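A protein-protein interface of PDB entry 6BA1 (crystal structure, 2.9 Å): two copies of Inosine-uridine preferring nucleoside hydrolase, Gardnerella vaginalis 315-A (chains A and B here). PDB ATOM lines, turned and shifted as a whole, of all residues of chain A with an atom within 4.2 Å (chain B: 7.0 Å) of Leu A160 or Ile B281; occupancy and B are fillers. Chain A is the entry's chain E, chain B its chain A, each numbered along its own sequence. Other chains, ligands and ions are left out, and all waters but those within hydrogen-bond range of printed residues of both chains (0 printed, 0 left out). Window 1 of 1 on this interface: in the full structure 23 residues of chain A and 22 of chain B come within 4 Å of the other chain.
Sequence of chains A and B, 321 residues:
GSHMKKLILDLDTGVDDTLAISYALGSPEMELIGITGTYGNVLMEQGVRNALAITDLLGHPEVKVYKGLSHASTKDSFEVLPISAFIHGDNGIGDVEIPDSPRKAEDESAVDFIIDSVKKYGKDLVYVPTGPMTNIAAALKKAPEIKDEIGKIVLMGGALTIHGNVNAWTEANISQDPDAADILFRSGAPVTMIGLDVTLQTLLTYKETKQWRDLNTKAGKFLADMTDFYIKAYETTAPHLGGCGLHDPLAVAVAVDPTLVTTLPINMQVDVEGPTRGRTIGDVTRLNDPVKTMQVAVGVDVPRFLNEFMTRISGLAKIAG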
ATOM      1  N   ALA A 159      25.685  -2.616  25.724  1.00  0.00           N
ATOM      2  CA  ALA A 159      24.401  -1.921  25.739  1.00  0.00           C
ATOM      3  C   ALA A 159      24.594  -0.598  25.011  1.00  0.00           C
ATOM      4  O   ALA A 159      25.379   0.235  25.465  1.00  0.00           O
ATOM      5  CB  ALA A 159      23.940  -1.680  27.163  1.00  0.00           C
ATOM      6  N   LEU A 160      23.918  -0.420  23.875  1.00  0.00           N
ATOM      7  CA  LEU A 160      24.090   0.782  23.061  1.00  0.00           C
ATOM      8  C   LEU A 160      23.160   1.867  23.543  1.00  0.00           C
ATOM      9  O   LEU A 160      23.621   2.888  24.040  1.00  0.00           O
ATOM     10  CB  LEU A 160      23.826   0.497  21.580  1.00  0.00           C
ATOM     11  CG  LEU A 160      23.965   1.687  20.621  1.00  0.00           C
ATOM     12  CD1 LEU A 160      25.376   2.254  20.666  1.00  0.00           C
ATOM     13  CD2 LEU A 160      23.603   1.265  19.209  1.00  0.00           C
ATOM     14  N   THR A 161      21.857   1.616  23.426  1.00  0.00           N
ATOM     15  CA  THR A 161      20.834   2.633  23.644  1.00  0.00           C
ATOM     16  C   THR A 161      20.272   2.646  25.066  1.00  0.00           C
ATOM     17  O   THR A 161      19.222   3.239  25.299  1.00  0.00           O
ATOM     18  CB  THR A 161      19.643   2.436  22.676  1.00  0.00           C
ATOM     19  OG1 THR A 161      18.873   1.299  23.082  1.00  0.00           O
ATOM     20  CG2 THR A 161      20.122   2.249  21.254  1.00  0.00           C
ATOM     21  N   ILE A 162      20.958   2.020  26.019  1.00  0.00           N
ATOM     22  CA  ILE A 162      20.379   1.811  27.341  1.00  0.00           C
ATOM     23  C   ILE A 162      21.449   1.673  28.428  1.00  0.00           C
ATOM     24  O   ILE A 162      22.640   1.572  28.127  1.00  0.00           O
ATOM     25  CB  ILE A 162      19.405   0.595  27.279  1.00  0.00           C
ATOM     26  CG1 ILE A 162      18.058   0.987  27.871  1.00  0.00           C
ATOM     27  CG2 ILE A 162      19.980  -0.692  27.896  1.00  0.00           C
ATOM     28  CD1 ILE A 162      17.055  -0.141  27.834  1.00  0.00           C
ATOM     29  N   HIS A 163      21.023   1.707  29.689  1.00  0.00           N
ATOM     30  CA  HIS A 163      21.939   1.492  30.809  1.00  0.00           C
ATOM     31  C   HIS A 163      22.500   0.071  30.805  1.00  0.00           C
ATOM     32  O   HIS A 163      21.770  -0.899  30.575  1.00  0.00           O
ATOM     33  CB  HIS A 163      21.247   1.707  32.159  1.00  0.00           C
ATOM     34  CG  HIS A 163      21.096   3.136  32.557  1.00  0.00           C
ATOM     35  ND1 HIS A 163      22.168   3.920  32.921  1.00  0.00           N
ATOM     36  CD2 HIS A 163      19.998   3.912  32.694  1.00  0.00           C
ATOM     37  CE1 HIS A 163      21.741   5.128  33.239  1.00  0.00           C
ATOM     38  NE2 HIS A 163      20.427   5.146  33.116  1.00  0.00           N
ATOM     39  N   MET A 193      26.264  -7.261  17.384  1.00  0.00           N
ATOM     40  CA  MET A 193      26.151  -7.140  18.835  1.00  0.00           C
ATOM     41  C   MET A 193      24.711  -7.367  19.258  1.00  0.00           C
ATOM     42  O   MET A 193      23.817  -6.715  18.741  1.00  0.00           O
ATOM     43  CB  MET A 193      26.621  -5.764  19.298  1.00  0.00           C
ATOM     44  CG  MET A 193      26.536  -5.544  20.798  1.00  0.00           C
ATOM     45  SD  MET A 193      27.113  -3.909  21.255  1.00  0.00           S
ATOM     46  CE  MET A 193      25.850  -3.443  22.433  1.00  0.00           C
ATOM     47  N   ASP A 197      19.848  -3.829  25.386  1.00  0.00           N
ATOM     48  CA  ASP A 197      18.746  -3.195  24.629  1.00  0.00           C
ATOM     49  C   ASP A 197      17.780  -4.171  23.941  1.00  0.00           C
ATOM     50  O   ASP A 197      16.620  -3.829  23.702  1.00  0.00           O
ATOM     51  CB  ASP A 197      19.246  -2.129  23.619  1.00  0.00           C
ATOM     52  CG  ASP A 197      20.652  -2.390  23.098  1.00  0.00           C
ATOM     53  OD1 ASP A 197      21.457  -1.433  23.112  1.00  0.00           O
ATOM     54  OD2 ASP A 197      20.958  -3.537  22.695  1.00  0.00           O
ATOM     55  N   LEU A 264      20.754  -2.050  13.775  1.00  0.00           N
ATOM     56  CA  LEU A 264      21.079  -0.695  13.368  1.00  0.00           C
ATOM     57  C   LEU A 264      22.502  -0.716  12.816  1.00  0.00           C
ATOM     58  O   LEU A 264      23.444  -0.876  13.583  1.00  0.00           O
ATOM     59  CB  LEU A 264      20.976   0.230  14.586  1.00  0.00           C
ATOM     60  CG  LEU A 264      21.655   1.609  14.569  1.00  0.00           C
ATOM     61  CD1 LEU A 264      21.224   2.452  13.374  1.00  0.00           C
ATOM     62  CD2 LEU A 264      21.380   2.329  15.875  1.00  0.00           C
ATOM     63  N   MET A 268      31.224   0.871  15.258  1.00  0.00           N
ATOM     64  CA  MET A 268      31.248   0.894  16.723  1.00  0.00           C
ATOM     65  C   MET A 268      32.654   0.914  17.309  1.00  0.00           C
ATOM     66  O   MET A 268      33.647   0.705  16.613  1.00  0.00           O
ATOM     67  CB  MET A 268      30.534  -0.340  17.262  1.00  0.00           C
ATOM     68  CG  MET A 268      29.032  -0.352  17.059  1.00  0.00           C
ATOM     69  SD  MET A 268      28.155   0.653  18.256  1.00  0.00           S
ATOM     70  CE  MET A 268      28.606  -0.136  19.799  1.00  0.00           C
ATOM     71  N   THR A 280      29.791   0.508  25.266  1.00  0.00           N
ATOM     72  CA  THR A 280      29.662   0.238  23.846  1.00  0.00           C
ATOM     73  C   THR A 280      28.983   1.440  23.205  1.00  0.00           C
ATOM     74  O   THR A 280      27.893   1.838  23.625  1.00  0.00           O
ATOM     75  CB  THR A 280      28.792  -0.998  23.618  1.00  0.00           C
ATOM     76  OG1 THR A 280      27.627  -0.899  24.443  1.00  0.00           O
ATOM     77  CG2 THR A 280      29.553  -2.263  23.984  1.00  0.00           C
ATOM     78  N   ILE A 281      29.624   2.019  22.196  1.00  0.00           N
ATOM     79  CA  ILE A 281      29.158   3.274  21.613  1.00  0.00           C
ATOM     80  C   ILE A 281      29.694   3.447  20.195  1.00  0.00           C
ATOM     81  O   ILE A 281      30.746   2.914  19.866  1.00  0.00           O
ATOM     82  CB  ILE A 281      29.575   4.462  22.519  1.00  0.00           C
ATOM     83  CG1 ILE A 281      28.784   5.729  22.182  1.00  0.00           C
ATOM     84  CG2 ILE A 281      31.079   4.721  22.463  1.00  0.00           C
ATOM     85  CD1 ILE A 281      27.317   5.646  22.536  1.00  0.00           C
ATOM     86  N   VAL A 296      24.168  -3.344  15.556  1.00  0.00           N
ATOM     87  CA  VAL A 296      23.697  -3.518  16.931  1.00  0.00           C
ATOM     88  C   VAL A 296      22.200  -3.771  16.931  1.00  0.00           C
ATOM     89  O   VAL A 296      21.448  -3.105  16.237  1.00  0.00           O
ATOM     90  CB  VAL A 296      24.011  -2.306  17.823  1.00  0.00           C
ATOM     91  CG1 VAL A 296      23.552  -2.568  19.256  1.00  0.00           C
ATOM     92  CG2 VAL A 296      25.503  -1.985  17.783  1.00  0.00           C
ATOM     93  N   ALA B 159      23.139  13.195  22.301  1.00  0.00           N
ATOM     94  CA  ALA B 159      23.788  12.220  21.429  1.00  0.00           C
ATOM     95  C   ALA B 159      23.506  10.838  22.004  1.00  0.00           C
ATOM     96  O   ALA B 159      23.927  10.549  23.122  1.00  0.00           O
ATOM     97  CB  ALA B 159      25.278  12.469  21.349  1.00  0.00           C
ATOM     98  N   LEU B 160      22.763  10.009  21.265  1.00  0.00           N
ATOM     99  CA  LEU B 160      22.365   8.691  21.757  1.00  0.00           C
ATOM    100  C   LEU B 160      23.438   7.679  21.441  1.00  0.00           C
ATOM    101  O   LEU B 160      24.066   7.148  22.351  1.00  0.00           O
ATOM    102  CB  LEU B 160      21.036   8.244  21.150  1.00  0.00           C
ATOM    103  CG  LEU B 160      20.517   6.866  21.591  1.00  0.00           C
ATOM    104  CD1 LEU B 160      20.291   6.819  23.085  1.00  0.00           C
ATOM    105  CD2 LEU B 160      19.238   6.515  20.868  1.00  0.00           C
ATOM    106  N   THR B 161      23.662   7.452  20.147  1.00  0.00           N
ATOM    107  CA  THR B 161      24.503   6.359  19.672  1.00  0.00           C
ATOM    108  C   THR B 161      25.954   6.766  19.416  1.00  0.00           C
ATOM    109  O   THR B 161      26.681   6.038  18.746  1.00  0.00           O
ATOM    110  CB  THR B 161      23.948   5.770  18.352  1.00  0.00           C
ATOM    111  OG1 THR B 161      24.189   6.687  17.272  1.00  0.00           O
ATOM    112  CG2 THR B 161      22.468   5.478  18.470  1.00  0.00           C
ATOM    113  N   ILE B 162      26.391   7.904  19.947  1.00  0.00           N
ATOM    114  CA  ILE B 162      27.685   8.460  19.566  1.00  0.00           C
ATOM    115  C   ILE B 162      28.270   9.357  20.664  1.00  0.00           C
ATOM    116  O   ILE B 162      27.591   9.680  21.644  1.00  0.00           O
ATOM    117  CB  ILE B 162      27.538   9.186  18.195  1.00  0.00           C
ATOM    118  CG1 ILE B 162      28.624   8.684  17.243  1.00  0.00           C
ATOM    119  CG2 ILE B 162      27.489  10.724  18.306  1.00  0.00           C
ATOM    120  CD1 ILE B 162      28.609   9.376  15.901  1.00  0.00           C
ATOM    121  N   PHE B 185      12.287  14.764  28.833  1.00  0.00           N
ATOM    122  CA  PHE B 185      12.305  13.432  28.211  1.00  0.00           C
ATOM    123  C   PHE B 185      11.351  12.494  28.947  1.00  0.00           C
ATOM    124  O   PHE B 185      10.534  11.804  28.319  1.00  0.00           O
ATOM    125  CB  PHE B 185      13.727  12.845  28.215  1.00  0.00           C
ATOM    126  CG  PHE B 185      14.669  13.435  27.184  1.00  0.00           C
ATOM    127  CD1 PHE B 185      14.486  14.703  26.641  1.00  0.00           C
ATOM    128  CD2 PHE B 185      15.784  12.712  26.788  1.00  0.00           C
ATOM    129  CE1 PHE B 185      15.386  15.211  25.711  1.00  0.00           C
ATOM    130  CE2 PHE B 185      16.686  13.224  25.861  1.00  0.00           C
ATOM    131  CZ  PHE B 185      16.485  14.470  25.324  1.00  0.00           C
ATOM    132  N   MET B 193      14.013  13.852  19.514  1.00  0.00           N
ATOM    133  CA  MET B 193      15.383  14.321  19.712  1.00  0.00           C
ATOM    134  C   MET B 193      16.143  14.259  18.398  1.00  0.00           C
ATOM    135  O   MET B 193      16.177  13.216  17.767  1.00  0.00           O
ATOM    136  CB  MET B 193      16.095  13.475  20.766  1.00  0.00           C
ATOM    137  CG  MET B 193      17.530  13.901  21.036  1.00  0.00           C
ATOM    138  SD  MET B 193      18.287  12.860  22.285  1.00  0.00           S
ATOM    139  CE  MET B 193      19.889  12.578  21.536  1.00  0.00           C
ATOM    140  N   LEU B 264      14.233   6.210  16.026  1.00  0.00           N
ATOM    141  CA  LEU B 264      14.205   4.981  16.796  1.00  0.00           C
ATOM    142  C   LEU B 264      13.248   5.193  17.966  1.00  0.00           C
ATOM    143  O   LEU B 264      13.577   5.943  18.880  1.00  0.00           O
ATOM    144  CB  LEU B 264      15.627   4.675  17.291  1.00  0.00           C
ATOM    145  CG  LEU B 264      15.843   3.700  18.459  1.00  0.00           C
ATOM    146  CD1 LEU B 264      15.200   2.345  18.205  1.00  0.00           C
ATOM    147  CD2 LEU B 264      17.328   3.536  18.711  1.00  0.00           C
ATOM    148  N   ILE B 266      11.842   5.031  21.381  1.00  0.00           N
ATOM    149  CA  ILE B 266      12.599   4.722  22.593  1.00  0.00           C
ATOM    150  C   ILE B 266      12.226   5.633  23.764  1.00  0.00           C
ATOM    151  O   ILE B 266      12.316   6.847  23.655  1.00  0.00           O
ATOM    152  CB  ILE B 266      14.126   4.811  22.327  1.00  0.00           C
ATOM    153  CG1 ILE B 266      14.936   4.431  23.576  1.00  0.00           C
ATOM    154  CG2 ILE B 266      14.535   6.198  21.825  1.00  0.00           C
ATOM    155  CD1 ILE B 266      16.424   4.338  23.308  1.00  0.00           C
ATOM    156  N   ASN B 267      11.812   5.037  24.878  1.00  0.00           N
ATOM    157  CA  ASN B 267      11.615   5.782  26.118  1.00  0.00           C
ATOM    158  C   ASN B 267      12.983   6.192  26.669  1.00  0.00           C
ATOM    159  O   ASN B 267      13.835   5.340  26.906  1.00  0.00           O
ATOM    160  CB  ASN B 267      10.835   4.950  27.141  1.00  0.00           C
ATOM    161  CG  ASN B 267       9.372   4.782  26.768  1.00  0.00           C
ATOM    162  OD1 ASN B 267       8.586   5.722  26.861  1.00  0.00           O
ATOM    163  ND2 ASN B 267       8.993   3.582  26.359  1.00  0.00           N
ATOM    164  N   MET B 268      13.171   7.497  26.866  1.00  0.00           N
ATOM    165  CA  MET B 268      14.477   8.097  27.151  1.00  0.00           C
ATOM    166  C   MET B 268      14.562   8.751  28.525  1.00  0.00           C
ATOM    167  O   MET B 268      13.560   8.941  29.212  1.00  0.00           O
ATOM    168  CB  MET B 268      14.786   9.163  26.106  1.00  0.00           C
ATOM    169  CG  MET B 268      15.078   8.632  24.717  1.00  0.00           C
ATOM    170  SD  MET B 268      16.744   8.014  24.536  1.00  0.00           S
ATOM    171  CE  MET B 268      17.720   9.467  24.891  1.00  0.00           C
ATOM    172  N   GLN B 269      15.792   9.086  28.898  1.00  0.00           N
ATOM    173  CA  GLN B 269      16.100   9.852  30.099  1.00  0.00           C
ATOM    174  C   GLN B 269      17.376  10.639  29.846  1.00  0.00           C
ATOM    175  O   GLN B 269      18.005  10.494  28.795  1.00  0.00           O
ATOM    176  CB  GLN B 269      16.296   8.927  31.309  1.00  0.00           C
ATOM    177  CG  GLN B 269      17.396   7.868  31.146  1.00  0.00           C
ATOM    178  CD  GLN B 269      17.792   7.193  32.445  1.00  0.00           C
ATOM    179  OE1 GLN B 269      17.093   6.317  32.943  1.00  0.00           O
ATOM    180  NE2 GLN B 269      18.930   7.584  32.990  1.00  0.00           N
ATOM    181  N   VAL B 270      17.750  11.468  30.808  1.00  0.00           N
ATOM    182  CA  VAL B 270      19.060  12.095  30.821  1.00  0.00           C
ATOM    183  C   VAL B 270      19.688  11.785  32.161  1.00  0.00           C
ATOM    184  O   VAL B 270      19.025  11.839  33.197  1.00  0.00           O
ATOM    185  CB  VAL B 270      18.994  13.618  30.589  1.00  0.00           C
ATOM    186  CG1 VAL B 270      20.375  14.256  30.714  1.00  0.00           C
ATOM    187  CG2 VAL B 270      18.388  13.912  29.223  1.00  0.00           C
ATOM    188  N   ASP B 271      20.968  11.439  32.125  1.00  0.00           N
ATOM    189  CA  ASP B 271      21.690  11.057  33.326  1.00  0.00           C
ATOM    190  C   ASP B 271      21.966  12.303  34.150  1.00  0.00           C
ATOM    191  O   ASP B 271      22.452  13.307  33.628  1.00  0.00           O
ATOM    192  CB  ASP B 271      22.991  10.316  32.985  1.00  0.00           C
ATOM    193  CG  ASP B 271      22.770   8.867  32.540  1.00  0.00           C
ATOM    194  OD1 ASP B 271      21.621   8.393  32.485  1.00  0.00           O
ATOM    195  OD2 ASP B 271      23.776   8.196  32.247  1.00  0.00           O
ATOM    196  N   THR B 276      28.460   9.903  34.297  1.00  0.00           N
ATOM    197  CA  THR B 276      27.871  10.153  32.983  1.00  0.00           C
ATOM    198  C   THR B 276      26.798  11.263  32.989  1.00  0.00           C
ATOM    199  O   THR B 276      25.960  11.302  32.091  1.00  0.00           O
ATOM    200  CB  THR B 276      27.220   8.871  32.435  1.00  0.00           C
ATOM    201  OG1 THR B 276      26.258   8.389  33.381  1.00  0.00           O
ATOM    202  CG2 THR B 276      28.259   7.809  32.192  1.00  0.00           C
ATOM    203  N   ARG B 279      24.304  12.799  29.867  1.00  0.00           N
ATOM    204  CA  ARG B 279      24.210  11.856  28.757  1.00  0.00           C
ATOM    205  C   ARG B 279      22.756  11.577  28.448  1.00  0.00           C
ATOM    206  O   ARG B 279      21.951  11.393  29.355  1.00  0.00           O
ATOM    207  CB  ARG B 279      24.957  10.551  29.104  1.00  0.00           C
ATOM    208  CG  ARG B 279      24.634   9.316  28.267  1.00  0.00           C
ATOM    209  CD  ARG B 279      25.784   8.320  28.284  1.00  0.00           C
ATOM    210  NE  ARG B 279      25.386   6.909  28.330  1.00  0.00           N
ATOM    211  CZ  ARG B 279      25.015   6.240  29.421  1.00  0.00           C
ATOM    212  NH1 ARG B 279      24.937   6.817  30.609  1.00  0.00           N
ATOM    213  NH2 ARG B 279      24.693   4.959  29.324  1.00  0.00           N
ATOM    214  N   THR B 280      22.434  11.551  27.163  1.00  0.00           N
ATOM    215  CA  THR B 280      21.119  11.153  26.691  1.00  0.00           C
ATOM    216  C   THR B 280      21.149   9.652  26.450  1.00  0.00           C
ATOM    217  O   THR B 280      21.998   9.156  25.701  1.00  0.00           O
ATOM    218  CB  THR B 280      20.794  11.854  25.373  1.00  0.00           C
ATOM    219  OG1 THR B 280      21.931  11.770  24.508  1.00  0.00           O
ATOM    220  CG2 THR B 280      20.482  13.329  25.611  1.00  0.00           C
ATOM    221  N   ILE B 281      20.233   8.924  27.083  1.00  0.00           N
ATOM    222  CA  ILE B 281      20.265   7.466  27.064  1.00  0.00           C
ATOM    223  C   ILE B 281      18.885   6.888  27.374  1.00  0.00           C
ATOM    224  O   ILE B 281      18.090   7.526  28.053  1.00  0.00           O
ATOM    225  CB  ILE B 281      21.324   6.951  28.071  1.00  0.00           C
ATOM    226  CG1 ILE B 281      21.679   5.481  27.813  1.00  0.00           C
ATOM    227  CG2 ILE B 281      20.883   7.155  29.520  1.00  0.00           C
ATOM    228  CD1 ILE B 281      22.430   5.260  26.516  1.00  0.00           C
ATOM    229  N   GLY B 282      18.600   5.694  26.859  1.00  0.00           N
ATOM    230  CA  GLY B 282      17.335   5.027  27.124  1.00  0.00           C
ATOM    231  C   GLY B 282      17.155   4.632  28.580  1.00  0.00           C
ATOM    232  O   GLY B 282      18.104   4.208  29.237  1.00  0.00           O
ATOM    233  N   ASP B 283      15.935   4.783  29.081  1.00  0.00           N
ATOM    234  CA  ASP B 283      15.596   4.342  30.425  1.00  0.00           C
ATOM    235  C   ASP B 283      15.251   2.872  30.338  1.00  0.00           C
ATOM    236  O   ASP B 283      14.374   2.481  29.558  1.00  0.00           O
ATOM    237  CB  ASP B 283      14.412   5.135  31.000  1.00  0.00           C
ATOM    238  CG  ASP B 283      14.152   4.831  32.474  1.00  0.00           C
ATOM    239  OD1 ASP B 283      13.043   5.141  32.953  1.00  0.00           O
ATOM    240  OD2 ASP B 283      15.043   4.286  33.163  1.00  0.00           O
ATOM    241  N   VAL B 284      15.940   2.069  31.146  1.00  0.00           N
ATOM    242  CA  VAL B 284      15.756   0.613  31.142  1.00  0.00           C
ATOM    243  C   VAL B 284      14.372   0.287  31.671  1.00  0.00           C
ATOM    244  O   VAL B 284      13.679  -0.563  31.112  1.00  0.00           O
ATOM    245  CB  VAL B 284      16.795  -0.137  32.009  1.00  0.00           C
ATOM    246  CG1 VAL B 284      16.715  -1.640  31.758  1.00  0.00           C
ATOM    247  CG2 VAL B 284      18.202   0.348  31.724  1.00  0.00           C
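A ring nitrogen (NE2) of His A163 is in hydrogen-bond range of the side-chain amide nitrogen (NE2) of Gln B269. The backbone NH (N) of Gly B282 lies within hydrogen-bond range of the backbone carbonyl oxygen (O) of Thr A161 (3.0 Å).
The side-chain sulfur of Met B268 is in hydrogen-bond range of the backbone NH of Gly B282, 3.8 Å away. NE2 of Gln B269 sits at hydrogen-bond distance from OD1 of Asp B271, at 2.9 Å. The side-chain carboxylate (OD2) of Asp B283 sits close to the side-chain amide oxygen (OE1) of Gln B269, at 2.9 Å. The side-chain hydroxyl (OG1) of Thr B276 sits at hydrogen-bond distance from the side-chain carboxylate (OD2) of Asp B271. The side-chain carboxylate (OD1) of Asp A197 is in hydrogen-bond range of the backbone NH (N) of Leu A160 (2.8 Å). The backbone NH (N) of Thr A161 lies within hydrogen-bond range of the side-chain carboxylate (OD1) of Asp A197.
O of Leu A160 touches CD1 of Ile B281, at 3.6 Å. Leu B264 touches Thr A161 (CD2 to CG2, 3.99 Å). CD1 of Ile B281 touches C of Thr A161, at 3.7 Å. Ile B281 touches Ile A162. Ile A162 touches Val B284 (CD1 to CA, 3.6 Å). His A163 touches Asp B271 (CE1 to OD1, 3.4 Å). Val B284 touches His A163 (CG2 to CB, 3.4 Å). Ile A281 touches Leu B160 (CD1 to O, 3.6 Å). CD1 of Ile A281 touches C of Thr B161, 3.6 Å away. Ile B162 touches Ile A281 (N to CD1, 3.6 Å).
Of chain B, only Ile B281 comes within 4 Å of Leu A160. Of chain A, only Leu A160 (3.6 Å), Thr A161 (3.7 Å) and Ile A162 (3.6 Å) come within 4 Å of Ile B281. Of the printed residues of chain A, Ile B162 touches Ile A281. Of the printed residues of chain A, Val B284 touches Ile A162 and His A163. Printed residues of chain B within 4 Å of Thr A161: Leu B264, Ile B266, Ile B281 and Gly B282. Of the printed residues of chain B, Ile A281 touches Leu B160 (3.6 Å), Thr B161 (3.6 Å) and Ile B162 (3.6 Å). Printed residues of chain A within 4 Å of Leu B264: Thr A161. Phe B185 touches none of the printed residues of chain A. The nearest printed residue of chain A that does not touch Leu B264 is Leu A264 (5.1 Å).
Of the 20 printed residues of chain B, 10 touch a printed residue of chain A. Hydrophobic or aromatic side chains of chain B within 4 Å of the printed part of chain A: Leu B264, Ile B266, Ile B281 and Val B284. Among the printed residues, no Asp or Glu carboxylate lies within 4 Å of a Lys or Arg side-chain nitrogen of the other chain.
Leu A160 touches Ile B281, and with the chains exchanged Ile A281 touches Leu B160. Thr A161 touches Leu B264, but with the chains exchanged Leu A264 does not touch Thr B161 (4.2 Å). Thr A161 touches Ile B281, and with the chains exchanged Ile A281 touches Thr B161. Ile A162 touches Ile B281, and with the chains exchanged Ile A281 touches Ile B162. 9 positions are printed for both chains. Of the 15 pairs that touch across the chains among the printed residues, 6 have their exchanged pair printed and touching as well.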
